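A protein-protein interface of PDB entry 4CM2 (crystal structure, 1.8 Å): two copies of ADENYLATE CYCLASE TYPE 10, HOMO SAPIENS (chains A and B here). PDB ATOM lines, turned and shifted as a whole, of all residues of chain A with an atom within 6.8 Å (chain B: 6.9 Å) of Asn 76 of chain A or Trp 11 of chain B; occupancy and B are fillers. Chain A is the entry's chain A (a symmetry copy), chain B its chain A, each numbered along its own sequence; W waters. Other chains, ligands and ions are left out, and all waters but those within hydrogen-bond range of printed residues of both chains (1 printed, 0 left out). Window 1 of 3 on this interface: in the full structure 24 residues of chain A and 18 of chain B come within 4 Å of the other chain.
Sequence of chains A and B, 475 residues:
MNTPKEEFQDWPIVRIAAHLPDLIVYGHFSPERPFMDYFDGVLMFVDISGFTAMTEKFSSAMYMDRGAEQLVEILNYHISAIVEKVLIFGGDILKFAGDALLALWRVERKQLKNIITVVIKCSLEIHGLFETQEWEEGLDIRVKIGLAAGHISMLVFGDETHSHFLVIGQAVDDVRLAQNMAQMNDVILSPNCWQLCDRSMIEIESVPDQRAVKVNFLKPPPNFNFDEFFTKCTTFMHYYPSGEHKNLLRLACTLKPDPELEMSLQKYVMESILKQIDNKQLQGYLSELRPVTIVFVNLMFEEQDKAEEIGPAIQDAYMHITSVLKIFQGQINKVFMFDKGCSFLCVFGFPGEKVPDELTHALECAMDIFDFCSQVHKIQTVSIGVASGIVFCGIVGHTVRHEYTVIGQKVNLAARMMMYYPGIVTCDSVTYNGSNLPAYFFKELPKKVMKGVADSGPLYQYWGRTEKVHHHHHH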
ATOM      1  N   GLN A  70      -7.681 -29.488  -4.942  1.00  0.00           N
ATOM      2  CA  GLN A  70      -6.505 -29.227  -4.111  1.00  0.00           C
ATOM      3  C   GLN A  70      -5.535 -28.276  -4.797  1.00  0.00           C
ATOM      4  O   GLN A  70      -4.931 -27.342  -4.186  1.00  0.00           O
ATOM      5  CB  GLN A  70      -5.818 -30.536  -3.800  1.00  0.00           C
ATOM      6  CG  GLN A  70      -6.552 -31.347  -2.745  1.00  0.00           C
ATOM      7  CD  GLN A  70      -5.752 -31.530  -1.494  1.00  0.00           C
ATOM      8  OE1 GLN A  70      -5.175 -30.591  -0.920  1.00  0.00           O
ATOM      9  NE2 GLN A  70      -5.766 -32.739  -1.027  1.00  0.00           N
ATOM     10  N   LEU A  71      -5.359 -28.498  -6.133  1.00  0.00           N
ATOM     11  CA  LEU A  71      -4.468 -27.597  -6.863  1.00  0.00           C
ATOM     12  C   LEU A  71      -4.884 -26.160  -6.854  1.00  0.00           C
ATOM     13  O   LEU A  71      -4.023 -25.276  -6.552  1.00  0.00           O
ATOM     14  CB  LEU A  71      -4.245 -28.081  -8.310  1.00  0.00           C
ATOM     15  CG  LEU A  71      -3.256 -27.231  -9.137  1.00  0.00           C
ATOM     16  CD1 LEU A  71      -1.861 -27.177  -8.540  1.00  0.00           C
ATOM     17  CD2 LEU A  71      -3.139 -27.914 -10.467  1.00  0.00           C
ATOM     18  N   VAL A  72      -6.108 -25.886  -7.166  1.00  0.00           N
ATOM     19  CA  VAL A  72      -6.627 -24.532  -7.182  1.00  0.00           C
ATOM     20  C   VAL A  72      -6.566 -23.891  -5.791  1.00  0.00           C
ATOM     21  O   VAL A  72      -6.225 -22.698  -5.689  1.00  0.00           O
ATOM     22  CB  VAL A  72      -7.984 -24.359  -7.874  1.00  0.00           C
ATOM     23  CG1 VAL A  72      -9.121 -24.902  -7.112  1.00  0.00           C
ATOM     24  CG2 VAL A  72      -8.363 -22.876  -8.015  1.00  0.00           C
ATOM     25  N   GLU A  73      -6.809 -24.694  -4.736  1.00  0.00           N
ATOM     26  CA  GLU A  73      -6.748 -24.146  -3.366  1.00  0.00           C
ATOM     27  C   GLU A  73      -5.304 -23.671  -3.027  1.00  0.00           C
ATOM     28  O   GLU A  73      -5.103 -22.546  -2.590  1.00  0.00           O
ATOM     29  CB  GLU A  73      -7.224 -25.249  -2.446  1.00  0.00           C
ATOM     30  CG  GLU A  73      -7.162 -24.858  -0.996  1.00  0.00           C
ATOM     31  CD  GLU A  73      -7.679 -25.920  -0.078  1.00  0.00           C
ATOM     32  OE1 GLU A  73      -7.688 -27.096  -0.558  1.00  0.00           O
ATOM     33  OE2 GLU A  73      -7.995 -25.585   1.085  1.00  0.00           O
ATOM     34  N   ILE A  74      -4.341 -24.500  -3.272  1.00  0.00           N
ATOM     35  CA  ILE A  74      -2.932 -24.201  -2.893  1.00  0.00           C
ATOM     36  C   ILE A  74      -2.363 -23.099  -3.813  1.00  0.00           C
ATOM     37  O   ILE A  74      -1.674 -22.200  -3.349  1.00  0.00           O
ATOM     38  CB  ILE A  74      -2.037 -25.437  -2.758  1.00  0.00           C
ATOM     39  CG1 ILE A  74      -0.756 -25.132  -2.038  1.00  0.00           C
ATOM     40  CG2 ILE A  74      -1.700 -26.071  -4.068  1.00  0.00           C
ATOM     41  CD1 ILE A  74      -0.952 -24.543  -0.647  1.00  0.00           C
ATOM     42  N   LEU A  75      -2.693 -23.164  -5.086  1.00  0.00           N
ATOM     43  CA  LEU A  75      -2.266 -22.078  -6.040  1.00  0.00           C
ATOM     44  C   LEU A  75      -2.847 -20.775  -5.630  1.00  0.00           C
ATOM     45  O   LEU A  75      -2.126 -19.737  -5.475  1.00  0.00           O
ATOM     46  CB  LEU A  75      -2.723 -22.300  -7.465  1.00  0.00           C
ATOM     47  CG  LEU A  75      -2.057 -23.449  -8.194  1.00  0.00           C
ATOM     48  CD1 LEU A  75      -2.657 -23.680  -9.593  1.00  0.00           C
ATOM     49  CD2 LEU A  75      -0.556 -23.270  -8.267  1.00  0.00           C
ATOM     50  N   ASN A  76      -4.145 -20.759  -5.381  1.00  0.00           N
ATOM     51  CA  ASN A  76      -4.744 -19.513  -4.969  1.00  0.00           C
ATOM     52  C   ASN A  76      -4.279 -18.943  -3.624  1.00  0.00           C
ATOM     53  O   ASN A  76      -4.196 -17.693  -3.427  1.00  0.00           O
ATOM     54  CB  ASN A  76      -6.254 -19.596  -5.052  1.00  0.00           C
ATOM     55  CG  ASN A  76      -6.727 -19.540  -6.509  1.00  0.00           C
ATOM     56  OD1 ASN A  76      -5.930 -19.265  -7.431  1.00  0.00           O
ATOM     57  ND2 ASN A  76      -7.964 -19.767  -6.699  1.00  0.00           N
ATOM     58  N   TYR A  77      -3.960 -19.818  -2.706  1.00  0.00           N
ATOM     59  CA  TYR A  77      -3.432 -19.389  -1.438  1.00  0.00           C
ATOM     60  C   TYR A  77      -2.094 -18.590  -1.638  1.00  0.00           C
ATOM     61  O   TYR A  77      -1.983 -17.449  -1.139  1.00  0.00           O
ATOM     62  CB  TYR A  77      -3.219 -20.574  -0.571  1.00  0.00           C
ATOM     63  CG  TYR A  77      -2.602 -20.234   0.755  1.00  0.00           C
ATOM     64  CD1 TYR A  77      -3.228 -19.382   1.653  1.00  0.00           C
ATOM     65  CD2 TYR A  77      -1.429 -20.765   1.075  1.00  0.00           C
ATOM     66  CE1 TYR A  77      -2.627 -19.117   2.876  1.00  0.00           C
ATOM     67  CE2 TYR A  77      -0.848 -20.539   2.307  1.00  0.00           C
ATOM     68  CZ  TYR A  77      -1.443 -19.659   3.164  1.00  0.00           C
ATOM     69  OH  TYR A  77      -0.768 -19.439   4.372  1.00  0.00           O
ATOM     70  N   HIS A  78      -1.209 -19.112  -2.470  1.00  0.00           N
ATOM     71  CA  HIS A  78       0.107 -18.458  -2.699  1.00  0.00           C
ATOM     72  C   HIS A  78      -0.036 -17.296  -3.641  1.00  0.00           C
ATOM     73  O   HIS A  78       0.576 -16.237  -3.363  1.00  0.00           O
ATOM     74  CB  HIS A  78       1.099 -19.467  -3.232  1.00  0.00           C
ATOM     75  CG  HIS A  78       1.521 -20.448  -2.165  1.00  0.00           C
ATOM     76  ND1 HIS A  78       1.891 -20.038  -0.899  1.00  0.00           N
ATOM     77  CD2 HIS A  78       1.517 -21.795  -2.130  1.00  0.00           C
ATOM     78  CE1 HIS A  78       2.136 -21.096  -0.147  1.00  0.00           C
ATOM     79  NE2 HIS A  78       1.936 -22.173  -0.869  1.00  0.00           N
ATOM     80  N   ILE A  79      -0.819 -17.472  -4.734  1.00  0.00           N
ATOM     81  CA  ILE A  79      -0.910 -16.390  -5.736  1.00  0.00           C
ATOM     82  C   ILE A  79      -1.647 -15.188  -5.090  1.00  0.00           C
ATOM     83  O   ILE A  79      -1.327 -14.003  -5.362  1.00  0.00           O
ATOM     84  CB  ILE A  79      -1.537 -16.859  -6.999  1.00  0.00           C
ATOM     85  CG1 ILE A  79      -0.599 -17.898  -7.658  1.00  0.00           C
ATOM     86  CG2 ILE A  79      -1.873 -15.690  -7.917  1.00  0.00           C
ATOM     87  CD1 ILE A  79      -1.203 -18.430  -8.864  1.00  0.00           C
ATOM     88  N   SER A  80      -2.665 -15.462  -4.264  1.00  0.00           N
ATOM     89  CA  SER A  80      -3.373 -14.376  -3.534  1.00  0.00           C
ATOM     90  C   SER A  80      -2.460 -13.440  -2.794  1.00  0.00           C
ATOM     91  O   SER A  80      -2.675 -12.214  -2.755  1.00  0.00           O
ATOM     92  CB  SER A  80      -4.381 -14.941  -2.499  1.00  0.00           C
ATOM     93  OG  SER A  80      -5.457 -15.240  -3.250  1.00  0.00           O
ATOM     94  N   ALA A  81      -1.471 -13.995  -2.152  1.00  0.00           N
ATOM     95  CA  ALA A  81      -0.542 -13.244  -1.391  1.00  0.00           C
ATOM     96  C   ALA A  81       0.296 -12.321  -2.312  1.00  0.00           C
ATOM     97  O   ALA A  81       0.618 -11.169  -1.942  1.00  0.00           O
ATOM     98  CB  ALA A  81       0.345 -14.157  -0.512  1.00  0.00           C
ATOM     99  N   GLY A 394      -9.107 -23.612 -14.256  1.00  0.00           N
ATOM    100  CA  GLY A 394      -9.756 -23.042 -13.082  1.00  0.00           C
ATOM    101  C   GLY A 394      -9.549 -21.555 -13.035  1.00  0.00           C
ATOM    102  O   GLY A 394      -8.728 -21.039 -13.720  1.00  0.00           O
ATOM    103  N   ILE A 395     -10.328 -20.911 -12.145  1.00  0.00           N
ATOM    104  CA  ILE A 395     -10.136 -19.483 -11.846  1.00  0.00           C
ATOM    105  C   ILE A 395      -9.016 -19.335 -10.811  1.00  0.00           C
ATOM    106  O   ILE A 395      -9.160 -19.756  -9.654  1.00  0.00           O
ATOM    107  CB  ILE A 395     -11.435 -18.807 -11.361  1.00  0.00           C
ATOM    108  CG1 ILE A 395     -12.482 -18.884 -12.507  1.00  0.00           C
ATOM    109  CG2 ILE A 395     -11.173 -17.389 -10.994  1.00  0.00           C
ATOM    110  CD1 ILE A 395     -13.909 -18.542 -12.078  1.00  0.00           C
ATOM    111  N   VAL A 396      -7.944 -18.729 -11.244  1.00  0.00           N
ATOM    112  CA  VAL A 396      -6.759 -18.555 -10.455  1.00  0.00           C
ATOM    113  C   VAL A 396      -6.492 -17.073 -10.091  1.00  0.00           C
ATOM    114  O   VAL A 396      -6.623 -16.198 -10.902  1.00  0.00           O
ATOM    115  CB  VAL A 396      -5.559 -19.051 -11.268  1.00  0.00           C
ATOM    116  CG1 VAL A 396      -4.236 -18.652 -10.589  1.00  0.00           C
ATOM    117  CG2 VAL A 396      -5.642 -20.571 -11.476  1.00  0.00           C
ATOM    118  N   GLY A 397      -6.155 -16.845  -8.810  1.00  0.00           N
ATOM    119  CA  GLY A 397      -5.799 -15.501  -8.307  1.00  0.00           C
ATOM    120  C   GLY A 397      -6.505 -15.241  -7.013  1.00  0.00           C
ATOM    121  O   GLY A 397      -6.776 -16.151  -6.215  1.00  0.00           O
ATOM    122  N   HIS A 398      -6.744 -13.973  -6.767  1.00  0.00           N
ATOM    123  CA  HIS A 398      -7.353 -13.464  -5.507  1.00  0.00           C
ATOM    124  C   HIS A 398      -8.833 -13.262  -5.761  1.00  0.00           C
ATOM    125  O   HIS A 398      -9.248 -12.958  -6.882  1.00  0.00           O
ATOM    126  CB  HIS A 398      -6.715 -12.116  -5.184  1.00  0.00           C
ATOM    127  CG  HIS A 398      -6.993 -11.581  -3.811  1.00  0.00           C
ATOM    128  ND1 HIS A 398      -8.186 -11.003  -3.431  1.00  0.00           N
ATOM    129  CD2 HIS A 398      -6.181 -11.515  -2.737  1.00  0.00           C
ATOM    130  CE1 HIS A 398      -8.119 -10.659  -2.160  1.00  0.00           C
ATOM    131  NE2 HIS A 398      -6.895 -10.902  -1.726  1.00  0.00           N
ATOM    132  N   HIS A 402      -8.664 -12.091 -10.405  1.00  0.00           N
ATOM    133  CA  HIS A 402      -8.449 -13.488 -10.767  1.00  0.00           C
ATOM    134  C   HIS A 402      -8.838 -13.733 -12.194  1.00  0.00           C
ATOM    135  O   HIS A 402      -9.506 -12.884 -12.796  1.00  0.00           O
ATOM    136  CB  HIS A 402      -9.183 -14.477  -9.852  1.00  0.00           C
ATOM    137  CG  HIS A 402     -10.650 -14.237  -9.684  1.00  0.00           C
ATOM    138  ND1 HIS A 402     -11.289 -14.635  -8.544  1.00  0.00           N
ATOM    139  CD2 HIS A 402     -11.610 -13.640 -10.450  1.00  0.00           C
ATOM    140  CE1 HIS A 402     -12.571 -14.256  -8.578  1.00  0.00           C
ATOM    141  NE2 HIS A 402     -12.809 -13.712  -9.753  1.00  0.00           N
ATOM    142  N   PHE B   8     -12.355 -13.270   5.193  1.00  0.00           N
ATOM    143  CA  PHE B   8     -12.948 -14.504   5.703  1.00  0.00           C
ATOM    144  C   PHE B   8     -12.352 -15.623   4.881  1.00  0.00           C
ATOM    145  O   PHE B   8     -12.615 -15.669   3.694  1.00  0.00           O
ATOM    146  CB  PHE B   8     -14.476 -14.438   5.487  1.00  0.00           C
ATOM    147  CG  PHE B   8     -15.211 -15.753   5.688  1.00  0.00           C
ATOM    148  CD1 PHE B   8     -14.797 -16.685   6.663  1.00  0.00           C
ATOM    149  CD2 PHE B   8     -16.363 -16.042   4.922  1.00  0.00           C
ATOM    150  CE1 PHE B   8     -15.488 -17.875   6.842  1.00  0.00           C
ATOM    151  CE2 PHE B   8     -17.064 -17.229   5.116  1.00  0.00           C
ATOM    152  CZ  PHE B   8     -16.624 -18.139   6.074  1.00  0.00           C
ATOM    153  N   GLN B   9     -11.490 -16.464   5.474  1.00  0.00           N
ATOM    154  CA  GLN B   9     -10.851 -17.525   4.752  1.00  0.00           C
ATOM    155  C   GLN B   9     -11.622 -18.917   4.867  1.00  0.00           C
ATOM    156  O   GLN B   9     -11.655 -19.581   5.882  1.00  0.00           O
ATOM    157  CB  GLN B   9      -9.379 -17.594   5.181  1.00  0.00           C
ATOM    158  CG  GLN B   9      -8.544 -16.389   4.718  1.00  0.00           C
ATOM    159  CD  GLN B   9      -7.123 -16.792   4.283  1.00  0.00           C
ATOM    160  OE1 GLN B   9      -6.417 -17.480   5.018  1.00  0.00           O
ATOM    161  NE2 GLN B   9      -6.712 -16.394   3.067  1.00  0.00           N
ATOM    162  N   ASP B  10     -12.286 -19.258   3.787  1.00  0.00           N
ATOM    163  CA  ASP B  10     -13.289 -20.325   3.729  1.00  0.00           C
ATOM    164  C   ASP B  10     -12.745 -21.401   2.790  1.00  0.00           C
ATOM    165  O   ASP B  10     -13.455 -21.939   1.939  1.00  0.00           O
ATOM    166  CB  ASP B  10     -14.469 -19.665   3.098  1.00  0.00           C
ATOM    167  CG  ASP B  10     -15.682 -20.512   3.099  1.00  0.00           C
ATOM    168  OD1 ASP B  10     -15.835 -21.456   3.888  1.00  0.00           O
ATOM    169  OD2 ASP B  10     -16.541 -20.122   2.293  1.00  0.00           O
ATOM    170  N   TRP B  11     -11.500 -21.703   2.963  1.00  0.00           N
ATOM    171  CA  TRP B  11     -10.846 -22.691   2.056  1.00  0.00           C
ATOM    172  C   TRP B  11     -11.461 -24.084   2.259  1.00  0.00           C
ATOM    173  O   TRP B  11     -11.909 -24.379   3.369  1.00  0.00           O
ATOM    174  CB  TRP B  11      -9.409 -22.762   2.544  1.00  0.00           C
ATOM    175  CG  TRP B  11      -8.555 -21.493   2.422  1.00  0.00           C
ATOM    176  CD1 TRP B  11      -8.117 -20.708   3.440  1.00  0.00           C
ATOM    177  CD2 TRP B  11      -8.140 -20.904   1.220  1.00  0.00           C
ATOM    178  NE1 TRP B  11      -7.367 -19.642   2.905  1.00  0.00           N
ATOM    179  CE2 TRP B  11      -7.401 -19.744   1.541  1.00  0.00           C
ATOM    180  CE3 TRP B  11      -8.346 -21.240  -0.135  1.00  0.00           C
ATOM    181  CZ2 TRP B  11      -6.851 -18.922   0.537  1.00  0.00           C
ATOM    182  CZ3 TRP B  11      -7.775 -20.447  -1.133  1.00  0.00           C
ATOM    183  CH2 TRP B  11      -7.042 -19.298  -0.777  1.00  0.00           C
ATOM    184  N   PRO B  12     -11.365 -24.985   1.281  1.00  0.00           N
ATOM    185  CA  PRO B  12     -11.748 -26.333   1.417  1.00  0.00           C
ATOM    186  C   PRO B  12     -11.187 -26.999   2.687  1.00  0.00           C
ATOM    187  O   PRO B  12     -11.889 -27.723   3.348  1.00  0.00           O
ATOM    188  CB  PRO B  12     -11.237 -26.978   0.086  1.00  0.00           C
ATOM    189  CG  PRO B  12     -11.347 -25.890  -0.874  1.00  0.00           C
ATOM    190  CD  PRO B  12     -10.972 -24.679  -0.156  1.00  0.00           C
ATOM    191  N   ILE B  13      -9.943 -26.784   3.064  1.00  0.00           N
ATOM    192  CA  ILE B  13      -9.409 -27.479   4.230  1.00  0.00           C
ATOM    193  C   ILE B  13     -10.177 -27.052   5.499  1.00  0.00           C
ATOM    194  O   ILE B  13     -10.357 -27.890   6.397  1.00  0.00           O
ATOM    195  CB  ILE B  13      -7.837 -27.297   4.346  1.00  0.00           C
ATOM    196  CG1 ILE B  13      -7.236 -28.312   5.331  1.00  0.00           C
ATOM    197  CG2 ILE B  13      -7.447 -25.847   4.672  1.00  0.00           C
ATOM    198  CD1 ILE B  13      -5.704 -28.247   5.281  1.00  0.00           C
ATOM    199  N   VAL B  14     -10.555 -25.793   5.563  1.00  0.00           N
ATOM    200  CA  VAL B  14     -11.345 -25.311   6.719  1.00  0.00           C
ATOM    201  C   VAL B  14     -12.714 -25.974   6.759  1.00  0.00           C
ATOM    202  O   VAL B  14     -13.220 -26.419   7.779  1.00  0.00           O
ATOM    203  CB  VAL B  14     -11.439 -23.772   6.682  1.00  0.00           C
ATOM    204  CG1 VAL B  14     -12.371 -23.286   7.687  1.00  0.00           C
ATOM    205  CG2 VAL B  14     -10.016 -23.179   6.870  1.00  0.00           C
ATOM    206  N   ARG B  15     -13.327 -26.034   5.616  1.00  0.00           N
ATOM    207  CA  ARG B  15     -14.642 -26.642   5.524  1.00  0.00           C
ATOM    208  C   ARG B  15     -14.613 -28.149   5.873  1.00  0.00           C
ATOM    209  O   ARG B  15     -15.531 -28.627   6.521  1.00  0.00           O
ATOM    210  CB  ARG B  15     -15.201 -26.454   4.097  1.00  0.00           C
ATOM    211  CG  ARG B  15     -15.485 -25.024   3.721  1.00  0.00           C
ATOM    212  CD  ARG B  15     -16.013 -25.037   2.257  1.00  0.00           C
ATOM    213  NE  ARG B  15     -16.605 -23.741   1.914  1.00  0.00           N
ATOM    214  CZ  ARG B  15     -17.434 -23.519   0.881  1.00  0.00           C
ATOM    215  NH1 ARG B  15     -17.803 -24.500   0.084  1.00  0.00           N
ATOM    216  NH2 ARG B  15     -17.971 -22.278   0.723  1.00  0.00           N
ATOM    217  N   ILE B  16     -13.569 -28.881   5.479  1.00  0.00           N
ATOM    218  CA  ILE B  16     -13.370 -30.263   5.829  1.00  0.00           C
ATOM    219  C   ILE B  16     -13.203 -30.372   7.360  1.00  0.00           C
ATOM    220  O   ILE B  16     -13.852 -31.216   8.022  1.00  0.00           O
ATOM    221  CB  ILE B  16     -12.172 -30.857   5.078  1.00  0.00           C
ATOM    222  CG1 ILE B  16     -12.557 -31.027   3.558  1.00  0.00           C
ATOM    223  CG2 ILE B  16     -11.786 -32.190   5.738  1.00  0.00           C
ATOM    224  CD1 ILE B  16     -11.414 -31.298   2.618  1.00  0.00           C
ATOM    225  N   ALA B  17     -12.430 -29.458   7.933  1.00  0.00           N
ATOM    226  CA  ALA B  17     -12.136 -29.517   9.390  1.00  0.00           C
ATOM    227  C   ALA B  17     -13.364 -29.280  10.254  1.00  0.00           C
ATOM    228  O   ALA B  17     -13.429 -29.757  11.410  1.00  0.00           O
ATOM    229  CB  ALA B  17     -11.092 -28.495   9.774  1.00  0.00           C
ATOM    230  N   CME B 253     -10.676 -22.980  12.463  1.00  0.00           N
ATOM    231  CA  CME B 253     -11.113 -21.948  11.521  1.00  0.00           C
ATOM    232  CB  CME B 253     -11.975 -20.870  12.212  1.00  0.00           C
ATOM    233  SG  CME B 253     -13.483 -21.545  12.896  1.00  0.00           S
ATOM    234  SD  CME B 253     -14.247 -22.731  11.347  1.00  0.00           S
ATOM    235  CE  CME B 253     -13.876 -24.329  12.046  1.00  0.00           C
ATOM    236  CZ  CME B 253     -13.518 -25.205  10.933  1.00  0.00           C
ATOM    237  OH  CME B 253     -14.587 -25.060   9.978  1.00  0.00           O
ATOM    238  C   CME B 253      -9.949 -21.141  10.894  1.00  0.00           C
ATOM    239  O   CME B 253     -10.124 -20.519   9.841  1.00  0.00           O
ATOM    240  N   THR B 254      -8.759 -21.279  11.429  1.00  0.00           N
ATOM    241  CA  THR B 254      -7.584 -20.607  10.960  1.00  0.00           C
ATOM    242  C   THR B 254      -6.676 -21.452  10.071  1.00  0.00           C
ATOM    243  O   THR B 254      -5.558 -21.041   9.718  1.00  0.00           O
ATOM    244  CB  THR B 254      -6.684 -20.099  12.129  1.00  0.00           C
ATOM    245  OG1 THR B 254      -5.974 -21.110  12.876  1.00  0.00           O
ATOM    246  CG2 THR B 254      -7.370 -19.180  13.095  1.00  0.00           C
ATOM    247  N   LEU B 255      -7.069 -22.695   9.812  1.00  0.00           N
ATOM    248  CA  LEU B 255      -6.254 -23.594   9.053  1.00  0.00           C
ATOM    249  C   LEU B 255      -5.969 -23.067   7.664  1.00  0.00           C
ATOM    250  O   LEU B 255      -6.862 -22.544   7.050  1.00  0.00           O
ATOM    251  CB  LEU B 255      -6.898 -24.994   8.935  1.00  0.00           C
ATOM    252  CG  LEU B 255      -6.824 -26.003  10.015  1.00  0.00           C
ATOM    253  CD1 LEU B 255      -7.655 -27.215   9.597  1.00  0.00           C
ATOM    254  CD2 LEU B 255      -5.397 -26.446  10.322  1.00  0.00           C
ATOM    255  N   LYS B 256      -4.738 -23.212   7.187  1.00  0.00           N
ATOM    256  CA  LYS B 256      -4.425 -22.742   5.843  1.00  0.00           C
ATOM    257  C   LYS B 256      -4.193 -23.929   4.949  1.00  0.00           C
ATOM    258  O   LYS B 256      -3.927 -25.022   5.426  1.00  0.00           O
ATOM    259  CB  LYS B 256      -3.229 -21.776   5.844  1.00  0.00           C
ATOM    260  CG  LYS B 256      -3.463 -20.567   6.760  1.00  0.00           C
ATOM    261  CD  LYS B 256      -4.627 -19.714   6.319  1.00  0.00           C
ATOM    262  CE  LYS B 256      -4.688 -18.554   7.329  1.00  0.00           C
ATOM    263  NZ  LYS B 256      -6.051 -18.098   7.415  1.00  0.00           N
ATOM    264  N   PRO B 257      -4.398 -23.747   3.632  1.00  0.00           N
ATOM    265  CA  PRO B 257      -4.073 -24.795   2.694  1.00  0.00           C
ATOM    266  C   PRO B 257      -2.803 -25.540   2.955  1.00  0.00           C
ATOM    267  O   PRO B 257      -1.711 -24.938   3.216  1.00  0.00           O
ATOM    268  CB  PRO B 257      -4.137 -24.076   1.353  1.00  0.00           C
ATOM    269  CG  PRO B 257      -5.269 -23.077   1.605  1.00  0.00           C
ATOM    270  CD  PRO B 257      -4.871 -22.554   2.932  1.00  0.00           C
ATOM    271  N   GLU B 262      -4.707 -31.921   4.078  1.00  0.00           N
ATOM    272  CA  GLU B 262      -6.057 -32.134   3.498  1.00  0.00           C
ATOM    273  C   GLU B 262      -6.233 -33.529   2.974  1.00  0.00           C
ATOM    274  O   GLU B 262      -7.338 -34.111   3.143  1.00  0.00           O
ATOM    275  CB  GLU B 262      -6.309 -31.153   2.375  1.00  0.00           C
ATOM    276  CG  GLU B 262      -7.692 -31.218   1.741  1.00  0.00           C
ATOM    277  CD  GLU B 262      -8.091 -30.027   0.879  1.00  0.00           C
ATOM    278  OE1 GLU B 262      -7.664 -28.872   1.250  1.00  0.00           O
ATOM    279  OE2 GLU B 262      -8.834 -30.259  -0.134  1.00  0.00           O
ATOM    280  N   ILE B 277     -18.576 -29.360  -0.358  1.00  0.00           N
ATOM    281  CA  ILE B 277     -17.423 -28.524   0.104  1.00  0.00           C
ATOM    282  C   ILE B 277     -16.689 -27.891  -1.078  1.00  0.00           C
ATOM    283  O   ILE B 277     -16.261 -26.727  -1.001  1.00  0.00           O
ATOM    284  CB  ILE B 277     -16.511 -29.348   0.990  1.00  0.00           C
ATOM    285  CG1 ILE B 277     -17.127 -29.457   2.419  1.00  0.00           C
ATOM    286  CG2 ILE B 277     -15.104 -28.724   1.066  1.00  0.00           C
ATOM    287  CD1 ILE B 277     -16.413 -30.384   3.320  1.00  0.00           C
HETATM  288  O   HOH W   1      -5.101 -27.733   1.355  1.00  0.00           O
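The side-chain amide nitrogen (ND2) of Asn 76 of chain A is in hydrogen-bond range of the backbone carbonyl oxygen (O) of Ile 395 of chain A (3.2 Å). The side-chain hydroxyl (OG) of Ser 80 of chain A lies within hydrogen-bond range of the backbone carbonyl oxygen (O) of Asn 76 of chain A (2.8 Å). The side-chain amide oxygen of Asn 76 of chain A lies within hydrogen-bond range of the backbone NH of Gly 397 of chain A (2.8 Å). NE1 of Trp 11 of chain B lies within hydrogen-bond range of OE1 of Gln 9 of chain B (3.2 Å). OE1 of Gln 9 of chain B lies within hydrogen-bond range of NZ of Lys 256 of chain B, at 2.5 Å.
Printed residues of chain B within 4 Å of Asn 76 of chain A: Trp 11. Of the printed residues of chain B, Tyr 77 of chain A touches Trp 11, Lys 256 and Pro 257. Of the printed residues of chain A, Trp 11 of chain B touches Glu 73, Asn 76 and Tyr 77. Printed residues of chain A within 4 Å of Pro 12 of chain B: Glu 73. Printed residues of chain A within 4 Å of Ile 13 of chain B: Glu 73 (3.0 Å). Of the printed residues of chain A, Lys 256 of chain B touches Tyr 77. Of the printed residues of chain A, Pro 257 of chain B touches Glu 73, Ile 74 and Tyr 77. The nearest printed residue of chain B that does not touch Asn 76 of chain A is Pro 257 of chain B (6.7 Å). The nearest printed residue of chain A that does not touch Trp 11 of chain B is Ser 80 of chain A (5.0 Å).
Water W1 lies within hydrogen-bond range of the side-chain carboxylate of Glu 262 of chain B (2.8 Å) and the side-chain carboxylate of Glu 73 of chain A (3.3 Å).
Hydrophobic or aromatic side chains of chain B that line the printed part of chain A: Trp 11, Pro 12, Ile 13 and Pro 257. Among the printed residues, no Asp or Glu carboxylate lies within 4 Å of a Lys or Arg side-chain nitrogen of the other chain.
Among the printed residues, pairs that only touch across the chains: Gln 70 of chain A with Glu 262 of chain B, Glu 73 of chain A with Trp 11 of chain B, Tyr 77 of chain A with Trp 11 of chain B, Glu 73 of chain A with Pro 257 of chain B, Tyr 77 of chain A with Lys 256 of chain B, Ile 74 of chain A with Pro 257 of chain B, Tyr 77 of chain A with Pro 257 of chain B and Asn 76 of chain A with Trp 11 of chain B.
The side-chain carboxylate (OE2) of Glu 73 of chain A lies close to the backbone nitrogen (N) of Pro 12 of chain B (3.4 Å). OE1 of Glu 262 of chain B lies close to OE1 of Glu 73 of chain A, 2.5 Å away. N of Ile 13 of chain B is in hydrogen-bond range of OE2 of Glu 73 of chain A.
No position is printed for both chains. Of the 11 pairs that touch across the chains among the printed residues, none has its exchanged pair printed and touching as well.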
